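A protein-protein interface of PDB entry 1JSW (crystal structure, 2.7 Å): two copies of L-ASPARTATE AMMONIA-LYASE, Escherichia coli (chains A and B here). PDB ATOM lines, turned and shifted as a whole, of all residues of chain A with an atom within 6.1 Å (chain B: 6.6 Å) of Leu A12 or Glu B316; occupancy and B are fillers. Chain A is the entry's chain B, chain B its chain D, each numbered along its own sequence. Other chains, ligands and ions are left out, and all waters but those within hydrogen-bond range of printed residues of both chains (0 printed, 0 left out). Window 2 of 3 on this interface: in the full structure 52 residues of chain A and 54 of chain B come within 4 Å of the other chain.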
ATOM      1  N   ASP A  10      13.719  -5.624   8.613  1.00  0.00           N
ATOM      2  CA  ASP A  10      14.484  -4.631   9.376  1.00  0.00           C
ATOM      3  C   ASP A  10      15.997  -4.772   9.136  1.00  0.00           C
ATOM      4  O   ASP A  10      16.445  -5.633   8.364  1.00  0.00           O
ATOM      5  CB  ASP A  10      14.188  -4.749  10.890  1.00  0.00           C
ATOM      6  CG  ASP A  10      14.946  -5.900  11.570  1.00  0.00           C
ATOM      7  OD1 ASP A  10      15.128  -6.975  10.956  1.00  0.00           O
ATOM      8  OD2 ASP A  10      15.348  -5.724  12.739  1.00  0.00           O
ATOM      9  N   LEU A  11      16.766  -3.949   9.850  1.00  0.00           N
ATOM     10  CA  LEU A  11      18.230  -3.940   9.769  1.00  0.00           C
ATOM     11  C   LEU A  11      18.743  -5.359   9.816  1.00  0.00           C
ATOM     12  O   LEU A  11      19.664  -5.720   9.094  1.00  0.00           O
ATOM     13  CB  LEU A  11      18.829  -3.168  10.956  1.00  0.00           C
ATOM     14  CG  LEU A  11      18.858  -1.639  11.017  1.00  0.00           C
ATOM     15  CD1 LEU A  11      19.909  -1.106  10.062  1.00  0.00           C
ATOM     16  CD2 LEU A  11      17.478  -1.035  10.753  1.00  0.00           C
ATOM     17  N   LEU A  12      18.131  -6.143  10.695  1.00  0.00           N
ATOM     18  CA  LEU A  12      18.488  -7.542  10.883  1.00  0.00           C
ATOM     19  C   LEU A  12      17.534  -8.487  10.140  1.00  0.00           C
ATOM     20  O   LEU A  12      16.727  -9.209  10.736  1.00  0.00           O
ATOM     21  CB  LEU A  12      18.552  -7.885  12.376  1.00  0.00           C
ATOM     22  CG  LEU A  12      19.757  -7.372  13.173  1.00  0.00           C
ATOM     23  CD1 LEU A  12      19.857  -5.850  13.163  1.00  0.00           C
ATOM     24  CD2 LEU A  12      19.631  -7.894  14.582  1.00  0.00           C
ATOM     25  N   GLY A  13      17.601  -8.405   8.819  1.00  0.00           N
ATOM     26  CA  GLY A  13      16.794  -9.251   7.979  1.00  0.00           C
ATOM     27  C   GLY A  13      15.294  -9.104   8.102  1.00  0.00           C
ATOM     28  O   GLY A  13      14.757  -8.111   8.598  1.00  0.00           O
ATOM     29  N   THR A  14      14.638 -10.178   7.683  1.00  0.00           N
ATOM     30  CA  THR A  14      13.193 -10.301   7.637  1.00  0.00           C
ATOM     31  C   THR A  14      12.711 -11.391   8.584  1.00  0.00           C
ATOM     32  O   THR A  14      13.174 -12.530   8.517  1.00  0.00           O
ATOM     33  CB  THR A  14      12.792 -10.732   6.218  1.00  0.00           C
ATOM     34  OG1 THR A  14      13.632 -11.830   5.816  1.00  0.00           O
ATOM     35  CG2 THR A  14      12.973  -9.582   5.225  1.00  0.00           C
ATOM     36  N   ARG A  15      11.773 -11.050   9.456  1.00  0.00           N
ATOM     37  CA  ARG A  15      11.225 -12.028  10.387  1.00  0.00           C
ATOM     38  C   ARG A  15       9.720 -11.920  10.204  1.00  0.00           C
ATOM     39  O   ARG A  15       9.234 -10.891   9.743  1.00  0.00           O
ATOM     40  CB  ARG A  15      11.644 -11.716  11.829  1.00  0.00           C
ATOM     41  CG  ARG A  15      13.123 -11.276  11.995  1.00  0.00           C
ATOM     42  CD  ARG A  15      14.148 -12.355  11.606  1.00  0.00           C
ATOM     43  NE  ARG A  15      15.457 -11.793  11.236  1.00  0.00           N
ATOM     44  CZ  ARG A  15      16.529 -12.516  10.874  1.00  0.00           C
ATOM     45  NH1 ARG A  15      16.463 -13.849  10.836  1.00  0.00           N
ATOM     46  NH2 ARG A  15      17.670 -11.907  10.530  1.00  0.00           N
ATOM     47  N   VAL A  25       8.425  -5.833  14.379  1.00  0.00           N
ATOM     48  CA  VAL A  25       9.641  -6.651  14.476  1.00  0.00           C
ATOM     49  C   VAL A  25      10.474  -6.321  15.704  1.00  0.00           C
ATOM     50  O   VAL A  25      10.650  -7.160  16.578  1.00  0.00           O
ATOM     51  CB  VAL A  25      10.587  -6.487  13.250  1.00  0.00           C
ATOM     52  CG1 VAL A  25      11.515  -7.677  13.144  1.00  0.00           C
ATOM     53  CG2 VAL A  25       9.810  -6.298  11.976  1.00  0.00           C
ATOM     54  N   ARG A  29      11.591  -9.071  18.298  1.00  0.00           N
ATOM     55  CA  ARG A  29      12.982  -9.420  18.592  1.00  0.00           C
ATOM     56  C   ARG A  29      13.278  -9.271  20.083  1.00  0.00           C
ATOM     57  O   ARG A  29      14.000 -10.086  20.668  1.00  0.00           O
ATOM     58  CB  ARG A  29      13.942  -8.545  17.768  1.00  0.00           C
ATOM     59  CG  ARG A  29      13.535  -8.416  16.306  1.00  0.00           C
ATOM     60  CD  ARG A  29      14.574  -7.708  15.450  1.00  0.00           C
ATOM     61  NE  ARG A  29      15.579  -8.625  14.916  1.00  0.00           N
ATOM     62  CZ  ARG A  29      15.559  -9.138  13.690  1.00  0.00           C
ATOM     63  NH1 ARG A  29      14.588  -8.835  12.845  1.00  0.00           N
ATOM     64  NH2 ARG A  29      16.520  -9.953  13.299  1.00  0.00           N
ATOM     65  N   LEU B 314      30.260  -8.003  20.500  1.00  0.00           N
ATOM     66  CA  LEU B 314      29.050  -8.704  20.905  1.00  0.00           C
ATOM     67  C   LEU B 314      28.081  -8.967  19.775  1.00  0.00           C
ATOM     68  O   LEU B 314      28.096  -8.287  18.744  1.00  0.00           O
ATOM     69  CB  LEU B 314      28.318  -7.916  21.994  1.00  0.00           C
ATOM     70  CG  LEU B 314      29.079  -7.481  23.248  1.00  0.00           C
ATOM     71  CD1 LEU B 314      28.285  -6.396  23.995  1.00  0.00           C
ATOM     72  CD2 LEU B 314      29.380  -8.674  24.143  1.00  0.00           C
ATOM     73  N   PRO B 315      27.240  -9.999  19.948  1.00  0.00           N
ATOM     74  CA  PRO B 315      26.228 -10.390  18.966  1.00  0.00           C
ATOM     75  C   PRO B 315      25.197  -9.273  18.735  1.00  0.00           C
ATOM     76  O   PRO B 315      24.827  -8.558  19.667  1.00  0.00           O
ATOM     77  CB  PRO B 315      25.607 -11.630  19.611  1.00  0.00           C
ATOM     78  CG  PRO B 315      26.777 -12.257  20.289  1.00  0.00           C
ATOM     79  CD  PRO B 315      27.394 -11.056  20.967  1.00  0.00           C
ATOM     80  N   GLU B 316      24.803  -9.099  17.473  1.00  0.00           N
ATOM     81  CA  GLU B 316      23.827  -8.087  17.063  1.00  0.00           C
ATOM     82  C   GLU B 316      22.439  -8.618  17.343  1.00  0.00           C
ATOM     83  O   GLU B 316      22.013  -9.588  16.730  1.00  0.00           O
ATOM     84  CB  GLU B 316      23.951  -7.815  15.567  1.00  0.00           C
ATOM     85  CG  GLU B 316      24.429  -6.434  15.222  1.00  0.00           C
ATOM     86  CD  GLU B 316      23.476  -5.719  14.283  1.00  0.00           C
ATOM     87  OE1 GLU B 316      23.065  -6.334  13.265  1.00  0.00           O
ATOM     88  OE2 GLU B 316      23.132  -4.540  14.572  1.00  0.00           O
ATOM     89  N   LEU B 317      21.721  -7.973  18.247  1.00  0.00           N
ATOM     90  CA  LEU B 317      20.391  -8.444  18.582  1.00  0.00           C
ATOM     91  C   LEU B 317      19.299  -7.484  18.158  1.00  0.00           C
ATOM     92  O   LEU B 317      18.258  -7.906  17.661  1.00  0.00           O
ATOM     93  CB  LEU B 317      20.292  -8.716  20.084  1.00  0.00           C
ATOM     94  CG  LEU B 317      21.412  -9.540  20.737  1.00  0.00           C
ATOM     95  CD1 LEU B 317      21.061  -9.761  22.194  1.00  0.00           C
ATOM     96  CD2 LEU B 317      21.625 -10.880  20.038  1.00  0.00           C
ATOM     97  N   GLN B 318      19.541  -6.193  18.336  1.00  0.00           N
ATOM     98  CA  GLN B 318      18.544  -5.195  17.979  1.00  0.00           C
ATOM     99  C   GLN B 318      18.720  -4.663  16.574  1.00  0.00           C
ATOM    100  O   GLN B 318      19.852  -4.494  16.112  1.00  0.00           O
ATOM    101  CB  GLN B 318      18.593  -4.023  18.963  1.00  0.00           C
ATOM    102  CG  GLN B 318      18.209  -4.386  20.387  1.00  0.00           C
ATOM    103  CD  GLN B 318      16.743  -4.751  20.521  1.00  0.00           C
ATOM    104  OE1 GLN B 318      16.049  -4.992  19.525  1.00  0.00           O
ATOM    105  NE2 GLN B 318      16.258  -4.783  21.762  1.00  0.00           N
ATOM    106  N   ALA B 319      17.595  -4.387  15.908  1.00  0.00           N
ATOM    107  CA  ALA B 319      17.605  -3.824  14.559  1.00  0.00           C
ATOM    108  C   ALA B 319      18.558  -2.635  14.642  1.00  0.00           C
ATOM    109  O   ALA B 319      18.303  -1.675  15.376  1.00  0.00           O
ATOM    110  CB  ALA B 319      16.215  -3.362  14.184  1.00  0.00           C
ATOM    111  N   GLY B 320      19.697  -2.748  13.961  1.00  0.00           N
ATOM    112  CA  GLY B 320      20.718  -1.706  14.002  1.00  0.00           C
ATOM    113  C   GLY B 320      20.405  -0.252  13.658  1.00  0.00           C
ATOM    114  O   GLY B 320      19.261   0.207  13.702  1.00  0.00           O
ATOM    115  N   SER B 321      21.463   0.491  13.348  1.00  0.00           N
ATOM    116  CA  SER B 321      21.342   1.896  12.988  1.00  0.00           C
ATOM    117  C   SER B 321      21.335   2.020  11.460  1.00  0.00           C
ATOM    118  O   SER B 321      22.099   1.326  10.778  1.00  0.00           O
ATOM    119  CB  SER B 321      22.510   2.696  13.598  1.00  0.00           C
ATOM    120  OG  SER B 321      23.776   2.239  13.136  1.00  0.00           O
ATOM    121  N   LYS B 327      27.442   1.494  16.178  1.00  0.00           N
ATOM    122  CA  LYS B 327      26.961   0.972  17.459  1.00  0.00           C
ATOM    123  C   LYS B 327      26.687  -0.539  17.502  1.00  0.00           C
ATOM    124  O   LYS B 327      26.261  -1.132  16.513  1.00  0.00           O
ATOM    125  CB  LYS B 327      25.667   1.701  17.850  1.00  0.00           C
ATOM    126  CG  LYS B 327      25.725   3.234  17.808  1.00  0.00           C
ATOM    127  CD  LYS B 327      24.416   3.877  18.323  1.00  0.00           C
ATOM    128  CE  LYS B 327      24.229   3.732  19.842  1.00  0.00           C
ATOM    129  NZ  LYS B 327      25.294   4.454  20.602  1.00  0.00           N
ATOM    130  N   VAL B 328      26.890  -1.129  18.682  1.00  0.00           N
ATOM    131  CA  VAL B 328      26.663  -2.555  18.947  1.00  0.00           C
ATOM    132  C   VAL B 328      26.350  -2.665  20.447  1.00  0.00           C
ATOM    133  O   VAL B 328      27.054  -3.356  21.192  1.00  0.00           O
ATOM    134  CB  VAL B 328      27.931  -3.424  18.615  1.00  0.00           C
ATOM    135  CG1 VAL B 328      27.664  -4.904  18.875  1.00  0.00           C
ATOM    136  CG2 VAL B 328      28.360  -3.222  17.163  1.00  0.00           C
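The side-chain carboxylate (OD1) of Asp A10 lies close to the backbone NH (N) of Leu A12.
O of Gly A13 lies close to OD1 of Asp A10, 2.6 Å away.
The side-chain carboxylate (OD1) of Asp A10 is in salt-bridge range of the guanidinium group (NH1) of Arg A29.
NH2 of Arg A15 lies within hydrogen-bond range of O of Leu A12 (2.9 Å).
O of Leu A12 lies within hydrogen-bond range of NH2 of Arg A29, 2.7 Å away.
Among the printed residues, pairs that only touch across the chains: Asp A10 with Ala B319, Leu A11 with Ala B319, Leu A11 with Gly B320, Leu A11 with Ser B321, Leu A12 with Glu B316, Leu A12 with Leu B317, Leu A12 with Gln B318, Leu A12 with Ala B319, Leu A12 with Gly B320 and Arg A29 with Leu B317.
Gly A13 touches none of the printed residues of chain B.
Glu B316 touches just one residue of chain A: Leu A12 (3.2 Å).
Of the printed residues of chain A, Leu B317 touches Leu A12 and Arg A29.
Of the printed residues of chain A, Gln B318 touches Leu A12.
Of the printed residues of chain A, Ser B321 touches Leu A11.
The nearest residue of chain B that does not touch Leu A12 is Ser B321 (6.5 Å).
The nearest printed residue of chain A that does not touch Ala B319 is Arg A29 (4.5 Å).
Printed residues of chain A that touch a printed residue of chain B: Asp A10, Leu A11, Leu A12 and Arg A29.
Among the printed residues, 10 pairs touch across the chains.
Among the printed residues, no Asp or Glu carboxylate lies within 4 Å of a Lys or Arg side-chain nitrogen of the other chain.
No position is printed for both chains.
Of the 10 pairs that touch across the chains among the printed residues, none has its exchanged pair printed and touching as well.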
